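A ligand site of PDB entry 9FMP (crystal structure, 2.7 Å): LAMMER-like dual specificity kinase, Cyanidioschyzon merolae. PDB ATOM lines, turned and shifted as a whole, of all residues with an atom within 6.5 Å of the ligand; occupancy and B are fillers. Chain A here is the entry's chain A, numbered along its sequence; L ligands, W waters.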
ATOM      1  N   LEU A  35     -22.462 -36.252  26.378  1.00  0.00           N
ATOM      2  CA  LEU A  35     -23.714 -35.607  26.032  1.00  0.00           C
ATOM      3  C   LEU A  35     -23.570 -34.468  25.033  1.00  0.00           C
ATOM      4  O   LEU A  35     -24.440 -34.298  24.182  1.00  0.00           O
ATOM      5  CB  LEU A  35     -24.411 -35.083  27.294  1.00  0.00           C
ATOM      6  CG  LEU A  35     -25.432 -36.041  27.905  1.00  0.00           C
ATOM      7  CD1 LEU A  35     -26.116 -35.413  29.109  1.00  0.00           C
ATOM      8  CD2 LEU A  35     -26.450 -36.453  26.861  1.00  0.00           C
ATOM      9  N   GLY A  36     -22.498 -33.692  25.104  1.00  0.00           N
ATOM     10  CA  GLY A  36     -22.342 -32.598  24.157  1.00  0.00           C
ATOM     11  C   GLY A  36     -21.016 -31.907  24.359  1.00  0.00           C
ATOM     12  O   GLY A  36     -20.248 -32.221  25.260  1.00  0.00           O
ATOM     13  N   SER A  37     -20.781 -30.911  23.497  1.00  0.00           N
ATOM     14  CA  SER A  37     -19.513 -30.213  23.497  1.00  0.00           C
ATOM     15  C   SER A  37     -19.727 -28.800  22.977  1.00  0.00           C
ATOM     16  O   SER A  37     -20.714 -28.507  22.296  1.00  0.00           O
ATOM     17  CB  SER A  37     -18.480 -30.962  22.645  1.00  0.00           C
ATOM     18  OG  SER A  37     -17.611 -30.061  21.973  1.00  0.00           O
ATOM     19  N   GLY A  38     -18.797 -27.915  23.326  1.00  0.00           N
ATOM     20  CA  GLY A  38     -18.838 -26.555  22.826  1.00  0.00           C
ATOM     21  C   GLY A  38     -17.569 -25.838  23.195  1.00  0.00           C
ATOM     22  O   GLY A  38     -16.687 -26.390  23.869  1.00  0.00           O
ATOM     23  N   PHE A  40     -17.160 -23.724  25.367  1.00  0.00           N
ATOM     24  CA  PHE A  40     -17.041 -23.673  26.812  1.00  0.00           C
ATOM     25  C   PHE A  40     -16.342 -24.906  27.384  1.00  0.00           C
ATOM     26  O   PHE A  40     -15.635 -24.810  28.384  1.00  0.00           O
ATOM     27  CB  PHE A  40     -18.417 -23.522  27.447  1.00  0.00           C
ATOM     28  CG  PHE A  40     -19.356 -24.651  27.121  1.00  0.00           C
ATOM     29  CD1 PHE A  40     -19.419 -25.775  27.928  1.00  0.00           C
ATOM     30  CD2 PHE A  40     -20.178 -24.581  26.000  1.00  0.00           C
ATOM     31  CE1 PHE A  40     -20.283 -26.811  27.626  1.00  0.00           C
ATOM     32  CE2 PHE A  40     -21.042 -25.617  25.698  1.00  0.00           C
ATOM     33  CZ  PHE A  40     -21.094 -26.739  26.513  1.00  0.00           C
ATOM     34  N   LYS A  42     -17.109 -29.400  27.783  1.00  0.00           N
ATOM     35  CA  LYS A  42     -17.805 -30.644  27.460  1.00  0.00           C
ATOM     36  C   LYS A  42     -18.923 -30.901  28.468  1.00  0.00           C
ATOM     37  O   LYS A  42     -18.743 -30.689  29.671  1.00  0.00           O
ATOM     38  CB  LYS A  42     -16.834 -31.849  27.442  1.00  0.00           C
ATOM     39  CG  LYS A  42     -15.536 -31.601  26.674  1.00  0.00           C
ATOM     40  CD  LYS A  42     -15.741 -31.606  25.173  1.00  0.00           C
ATOM     41  CE  LYS A  42     -15.710 -33.020  24.613  1.00  0.00           C
ATOM     42  NZ  LYS A  42     -14.357 -33.633  24.742  1.00  0.00           N
ATOM     43  N   VAL A  43     -20.061 -31.364  27.978  1.00  0.00           N
ATOM     44  CA  VAL A  43     -21.194 -31.770  28.815  1.00  0.00           C
ATOM     45  C   VAL A  43     -21.256 -33.287  28.799  1.00  0.00           C
ATOM     46  O   VAL A  43     -21.225 -33.908  27.726  1.00  0.00           O
ATOM     47  CB  VAL A  43     -22.511 -31.147  28.340  1.00  0.00           C
ATOM     48  CG1 VAL A  43     -23.631 -31.523  29.304  1.00  0.00           C
ATOM     49  CG2 VAL A  43     -22.386 -29.646  28.230  1.00  0.00           C
ATOM     50  N   VAL A  55     -27.798 -37.039  36.005  1.00  0.00           N
ATOM     51  CA  VAL A  55     -27.615 -35.608  35.885  1.00  0.00           C
ATOM     52  C   VAL A  55     -26.747 -35.333  34.673  1.00  0.00           C
ATOM     53  O   VAL A  55     -26.146 -36.236  34.085  1.00  0.00           O
ATOM     54  CB  VAL A  55     -26.998 -34.985  37.154  1.00  0.00           C
ATOM     55  CG1 VAL A  55     -27.970 -35.075  38.324  1.00  0.00           C
ATOM     56  CG2 VAL A  55     -25.679 -35.678  37.482  1.00  0.00           C
ATOM     57  N   ALA A  56     -26.680 -34.060  34.289  1.00  0.00           N
ATOM     58  CA  ALA A  56     -25.806 -33.618  33.202  1.00  0.00           C
ATOM     59  C   ALA A  56     -24.801 -32.650  33.787  1.00  0.00           C
ATOM     60  O   ALA A  56     -25.175 -31.586  34.287  1.00  0.00           O
ATOM     61  CB  ALA A  56     -26.608 -32.970  32.087  1.00  0.00           C
ATOM     62  N   LYS A  58     -21.832 -30.139  33.144  1.00  0.00           N
ATOM     63  CA  LYS A  58     -21.163 -29.296  32.168  1.00  0.00           C
ATOM     64  C   LYS A  58     -19.833 -28.867  32.786  1.00  0.00           C
ATOM     65  O   LYS A  58     -19.806 -28.141  33.784  1.00  0.00           O
ATOM     66  CB  LYS A  58     -22.045 -28.095  31.818  1.00  0.00           C
ATOM     67  CG  LYS A  58     -21.405 -27.010  30.991  1.00  0.00           C
ATOM     68  CD  LYS A  58     -22.447 -25.982  30.581  1.00  0.00           C
ATOM     69  CE  LYS A  58     -21.815 -24.706  30.051  1.00  0.00           C
ATOM     70  NZ  LYS A  58     -22.808 -23.787  29.435  1.00  0.00           N
ATOM     71  N   VAL A  92     -33.625 -24.486  31.597  1.00  0.00           N
ATOM     72  CA  VAL A  92     -32.962 -25.639  32.180  1.00  0.00           C
ATOM     73  C   VAL A  92     -32.734 -25.415  33.673  1.00  0.00           C
ATOM     74  O   VAL A  92     -32.318 -24.327  34.095  1.00  0.00           O
ATOM     75  CB  VAL A  92     -31.655 -25.960  31.438  1.00  0.00           C
ATOM     76  CG1 VAL A  92     -30.640 -24.834  31.597  1.00  0.00           C
ATOM     77  CG2 VAL A  92     -31.072 -27.295  31.896  1.00  0.00           C
ATOM     78  N   PHE A 113     -26.821 -29.933  35.928  1.00  0.00           N
ATOM     79  CA  PHE A 113     -28.181 -29.687  35.473  1.00  0.00           C
ATOM     80  C   PHE A 113     -28.998 -30.978  35.505  1.00  0.00           C
ATOM     81  O   PHE A 113     -28.450 -32.086  35.568  1.00  0.00           O
ATOM     82  CB  PHE A 113     -28.210 -29.163  34.021  1.00  0.00           C
ATOM     83  CG  PHE A 113     -27.289 -28.009  33.763  1.00  0.00           C
ATOM     84  CD1 PHE A 113     -25.963 -28.226  33.437  1.00  0.00           C
ATOM     85  CD2 PHE A 113     -27.769 -26.718  33.805  1.00  0.00           C
ATOM     86  CE1 PHE A 113     -25.121 -27.168  33.177  1.00  0.00           C
ATOM     87  CE2 PHE A 113     -26.921 -25.652  33.547  1.00  0.00           C
ATOM     88  CZ  PHE A 113     -25.600 -25.880  33.232  1.00  0.00           C
ATOM     89  N   GLU A 114     -30.313 -30.802  35.427  1.00  0.00           N
ATOM     90  CA  GLU A 114     -31.208 -31.897  35.101  1.00  0.00           C
ATOM     91  C   GLU A 114     -30.785 -32.552  33.791  1.00  0.00           C
ATOM     92  O   GLU A 114     -30.344 -31.881  32.855  1.00  0.00           O
ATOM     93  CB  GLU A 114     -32.644 -31.397  34.994  1.00  0.00           C
ATOM     94  CG  GLU A 114     -32.787 -30.195  34.066  1.00  0.00           C
ATOM     95  CD  GLU A 114     -34.230 -29.904  33.681  1.00  0.00           C
ATOM     96  OE1 GLU A 114     -35.128 -30.669  34.100  1.00  0.00           O
ATOM     97  OE2 GLU A 114     -34.461 -28.910  32.960  1.00  0.00           O
ATOM     98  N   HIS A 115     -30.959 -33.864  33.724  1.00  0.00           N
ATOM     99  CA  HIS A 115     -30.547 -34.635  32.550  1.00  0.00           C
ATOM    100  C   HIS A 115     -31.651 -34.577  31.491  1.00  0.00           C
ATOM    101  O   HIS A 115     -32.750 -35.087  31.703  1.00  0.00           O
ATOM    102  CB  HIS A 115     -30.257 -36.084  32.943  1.00  0.00           C
ATOM    103  CG  HIS A 115     -29.472 -36.833  31.904  1.00  0.00           C
ATOM    104  ND1 HIS A 115     -29.930 -37.007  30.623  1.00  0.00           N
ATOM    105  CD2 HIS A 115     -28.271 -37.443  31.974  1.00  0.00           C
ATOM    106  CE1 HIS A 115     -29.043 -37.697  29.930  1.00  0.00           C
ATOM    107  NE2 HIS A 115     -28.024 -37.982  30.731  1.00  0.00           N
ATOM    108  N   LEU A 116     -31.331 -33.979  30.347  1.00  0.00           N
ATOM    109  CA  LEU A 116     -32.272 -33.806  29.249  1.00  0.00           C
ATOM    110  C   LEU A 116     -31.857 -34.668  28.054  1.00  0.00           C
ATOM    111  O   LEU A 116     -30.800 -35.305  28.064  1.00  0.00           O
ATOM    112  CB  LEU A 116     -32.378 -32.335  28.845  1.00  0.00           C
ATOM    113  CG  LEU A 116     -32.725 -31.334  29.954  1.00  0.00           C
ATOM    114  CD1 LEU A 116     -32.916 -29.942  29.368  1.00  0.00           C
ATOM    115  CD2 LEU A 116     -33.972 -31.778  30.704  1.00  0.00           C
ATOM    116  N   GLY A 117     -32.706 -34.672  27.038  1.00  0.00           N
ATOM    117  CA  GLY A 117     -32.451 -35.433  25.837  1.00  0.00           C
ATOM    118  C   GLY A 117     -31.607 -34.682  24.839  1.00  0.00           C
ATOM    119  O   GLY A 117     -30.816 -33.795  25.188  1.00  0.00           O
ATOM    120  N   PRO A 118     -31.762 -35.010  23.562  1.00  0.00           N
ATOM    121  CA  PRO A 118     -30.917 -34.420  22.530  1.00  0.00           C
ATOM    122  C   PRO A 118     -31.387 -33.014  22.176  1.00  0.00           C
ATOM    123  O   PRO A 118     -32.477 -32.570  22.546  1.00  0.00           O
ATOM    124  CB  PRO A 118     -31.075 -35.371  21.329  1.00  0.00           C
ATOM    125  CG  PRO A 118     -32.086 -36.434  21.767  1.00  0.00           C
ATOM    126  CD  PRO A 118     -32.772 -35.918  22.989  1.00  0.00           C
ATOM    127  N   SER A 119     -30.533 -32.304  21.439  1.00  0.00           N
ATOM    128  CA  SER A 119     -30.844 -30.947  21.033  1.00  0.00           C
ATOM    129  C   SER A 119     -31.716 -30.946  19.790  1.00  0.00           C
ATOM    130  O   SER A 119     -31.919 -31.969  19.125  1.00  0.00           O
ATOM    131  CB  SER A 119     -29.562 -30.168  20.747  1.00  0.00           C
ATOM    132  OG  SER A 119     -29.124 -30.394  19.426  1.00  0.00           O
ATOM    133  N   ASP A 122     -29.570 -31.898  17.102  1.00  0.00           N
ATOM    134  CA  ASP A 122     -29.454 -33.354  17.028  1.00  0.00           C
ATOM    135  C   ASP A 122     -30.629 -33.949  16.263  1.00  0.00           C
ATOM    136  O   ASP A 122     -30.443 -34.869  15.447  1.00  0.00           O
ATOM    137  CB  ASP A 122     -29.380 -33.942  18.436  1.00  0.00           C
ATOM    138  CG  ASP A 122     -28.053 -33.673  19.117  1.00  0.00           C
ATOM    139  OD1 ASP A 122     -27.019 -33.630  18.418  1.00  0.00           O
ATOM    140  OD2 ASP A 122     -28.054 -33.492  20.357  1.00  0.00           O
ATOM    141  N   LYS A 163     -29.868 -20.731  19.493  1.00  0.00           N
ATOM    142  CA  LYS A 163     -29.435 -21.584  18.396  1.00  0.00           C
ATOM    143  C   LYS A 163     -30.068 -22.950  18.596  1.00  0.00           C
ATOM    144  O   LYS A 163     -30.450 -23.297  19.716  1.00  0.00           O
ATOM    145  CB  LYS A 163     -27.903 -21.690  18.345  1.00  0.00           C
ATOM    146  CG  LYS A 163     -27.317 -22.610  19.403  1.00  0.00           C
ATOM    147  CD  LYS A 163     -26.068 -22.048  20.029  1.00  0.00           C
ATOM    148  CE  LYS A 163     -24.821 -22.422  19.265  1.00  0.00           C
ATOM    149  NZ  LYS A 163     -23.610 -22.114  20.067  1.00  0.00           N
ATOM    150  N   GLU A 165     -28.760 -25.772  18.858  1.00  0.00           N
ATOM    151  CA  GLU A 165     -28.007 -26.576  19.818  1.00  0.00           C
ATOM    152  C   GLU A 165     -28.406 -26.298  21.256  1.00  0.00           C
ATOM    153  O   GLU A 165     -28.178 -27.149  22.124  1.00  0.00           O
ATOM    154  CB  GLU A 165     -26.507 -26.336  19.637  1.00  0.00           C
ATOM    155  CG  GLU A 165     -25.915 -26.937  18.364  1.00  0.00           C
ATOM    156  CD  GLU A 165     -25.561 -25.892  17.318  1.00  0.00           C
ATOM    157  OE1 GLU A 165     -26.397 -25.005  17.040  1.00  0.00           O
ATOM    158  OE2 GLU A 165     -24.438 -25.968  16.763  1.00  0.00           O
ATOM    159  N   ASN A 166     -28.991 -25.128  21.539  1.00  0.00           N
ATOM    160  CA  ASN A 166     -29.361 -24.736  22.892  1.00  0.00           C
ATOM    161  C   ASN A 166     -30.849 -24.938  23.173  1.00  0.00           C
ATOM    162  O   ASN A 166     -31.374 -24.352  24.127  1.00  0.00           O
ATOM    163  CB  ASN A 166     -28.955 -23.297  23.163  1.00  0.00           C
ATOM    164  CG  ASN A 166     -27.459 -23.125  23.287  1.00  0.00           C
ATOM    165  OD1 ASN A 166     -26.728 -24.108  23.445  1.00  0.00           O
ATOM    166  ND2 ASN A 166     -26.992 -21.888  23.227  1.00  0.00           N
ATOM    167  N   VAL A 167     -31.533 -25.730  22.367  1.00  0.00           N
ATOM    168  CA  VAL A 167     -32.903 -26.163  22.645  1.00  0.00           C
ATOM    169  C   VAL A 167     -32.870 -27.678  22.758  1.00  0.00           C
ATOM    170  O   VAL A 167     -32.517 -28.360  21.798  1.00  0.00           O
ATOM    171  CB  VAL A 167     -33.885 -25.714  21.560  1.00  0.00           C
ATOM    172  CG1 VAL A 167     -35.296 -26.112  21.940  1.00  0.00           C
ATOM    173  CG2 VAL A 167     -33.769 -24.212  21.332  1.00  0.00           C
ATOM    174  N   LEU A 168     -33.213 -28.197  23.935  1.00  0.00           N
ATOM    175  CA  LEU A 168     -33.138 -29.623  24.198  1.00  0.00           C
ATOM    176  C   LEU A 168     -34.531 -30.228  24.366  1.00  0.00           C
ATOM    177  O   LEU A 168     -35.471 -29.549  24.777  1.00  0.00           O
ATOM    178  CB  LEU A 168     -32.304 -29.916  25.450  1.00  0.00           C
ATOM    179  CG  LEU A 168     -30.899 -29.318  25.502  1.00  0.00           C
ATOM    180  CD1 LEU A 168     -30.155 -29.869  26.709  1.00  0.00           C
ATOM    181  CD2 LEU A 168     -30.124 -29.601  24.243  1.00  0.00           C
ATOM    182  N   ILE A 189     -31.350 -23.814  27.103  1.00  0.00           N
ATOM    183  CA  ILE A 189     -30.154 -24.008  27.915  1.00  0.00           C
ATOM    184  C   ILE A 189     -29.117 -22.947  27.557  1.00  0.00           C
ATOM    185  O   ILE A 189     -29.339 -22.082  26.715  1.00  0.00           O
ATOM    186  CB  ILE A 189     -29.562 -25.419  27.750  1.00  0.00           C
ATOM    187  CG1 ILE A 189     -28.988 -25.573  26.341  1.00  0.00           C
ATOM    188  CG2 ILE A 189     -30.595 -26.479  28.049  1.00  0.00           C
ATOM    189  CD1 ILE A 189     -28.134 -26.804  26.158  1.00  0.00           C
ATOM    190  N   ASP A 190     -27.967 -23.047  28.223  1.00  0.00           N
ATOM    191  CA  ASP A 190     -26.778 -22.245  27.978  1.00  0.00           C
ATOM    192  C   ASP A 190     -27.005 -20.774  28.291  1.00  0.00           C
ATOM    193  O   ASP A 190     -27.390 -19.991  27.410  1.00  0.00           O
ATOM    194  CB  ASP A 190     -26.291 -22.407  26.533  1.00  0.00           C
ATOM    195  CG  ASP A 190     -24.806 -22.118  26.383  1.00  0.00           C
ATOM    196  OD1 ASP A 190     -24.219 -21.516  27.314  1.00  0.00           O
ATOM    197  OD2 ASP A 190     -24.220 -22.504  25.354  1.00  0.00           O
HETATM  198  O1  LIG L   1     -24.073 -26.528  24.479  1.00  0.00           O
HETATM  199  C1  LIG L   1     -24.550 -27.655  25.218  1.00  0.00           C
HETATM  200  C2  LIG L   1     -24.249 -28.955  24.509  1.00  0.00           C
HETATM  201  O2  LIG L   1     -24.295 -30.026  25.480  1.00  0.00           O
HETATM  202  C3  LIG L   1     -25.227 -29.357  23.430  1.00  0.00           C
HETATM  203  O3  LIG L   1     -24.588 -30.256  22.523  1.00  0.00           O
HETATM  204  C4  LIG L   1     -26.315 -30.101  24.206  1.00  0.00           C
HETATM  205  O4  LIG L   1     -26.990 -31.101  23.476  1.00  0.00           O
HETATM  206  C5  LIG L   1     -25.538 -30.705  25.395  1.00  0.00           C
HETATM  207  N1  LIG L   1     -26.233 -30.539  26.681  1.00  0.00           N
HETATM  208  C6  LIG L   1     -26.133 -29.482  27.539  1.00  0.00           C
HETATM  209  N2  LIG L   1     -26.873 -29.594  28.616  1.00  0.00           N
HETATM  210  C7  LIG L   1     -27.497 -30.817  28.452  1.00  0.00           C
HETATM  211  C8  LIG L   1     -28.420 -31.526  29.253  1.00  0.00           C
HETATM  212  N3  LIG L   1     -28.886 -31.083  30.419  1.00  0.00           N
HETATM  213  N4  LIG L   1     -28.857 -32.725  28.797  1.00  0.00           N
HETATM  214  C9  LIG L   1     -28.396 -33.177  27.629  1.00  0.00           C
HETATM  215  N5  LIG L   1     -27.533 -32.600  26.784  1.00  0.00           N
HETATM  216  C10 LIG L   1     -27.117 -31.418  27.264  1.00  0.00           C
HETATM  217  O   HOH W   1     -27.466 -27.528  30.462  1.00  0.00           O
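The backbone carbonyl oxygen (O) of Glu 114 is in hydrogen-bond range of a nitrogen (N3) of the ligand (2.9 Å).
The backbone NH (N) of Leu 116 is in hydrogen-bond range of a nitrogen (N4) of the ligand.
O of Gly 36 lies within hydrogen-bond range of N of Val 43.
O of Val 43 sits at hydrogen-bond distance from N of Leu 35, at 3.0 Å.
N of Phe 113 lies within hydrogen-bond range of O of Ala 56, at 2.9 Å.
The backbone NH (N) of Ile 189 sits at hydrogen-bond distance from the backbone carbonyl oxygen (O) of Asn 166 (3.0 Å).
N of Asp 122 sits at hydrogen-bond distance from OG of Ser 119 (2.8 Å).
Leu 35 touches the ligand (CD1 to C9, 3.5 Å).
Gly 36 touches the ligand.
Ser 37 touches the ligand (N to O3, 3.98 Å).
CE2 of Phe 40 touches O1 of the ligand, at 3.4 Å.
Val 43 touches the ligand (CG2 to O2, 3.4 Å).
CB of Ala 56 touches N3 of the ligand (3.4 Å).
Gly 117 touches the ligand (O to C9, 3.5 Å).
Ser 119 touches the ligand.
O of Glu 165 touches C3 of the ligand, 3.9 Å away.
Asn 166 touches the ligand (OD1 to O1, 3.7 Å).
Leu 168 touches the ligand (CD1 to C7, 3.3 Å).
Ile 189 touches the ligand.
Hydrophobic or aromatic side chains within 4 Å of the ligand: Leu 35, Phe 40, Val 43, Ala 56, Leu 116, Leu 168 and Ile 189.
Of the 26 residues printed, 14 come within 4 Å of the ligand.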
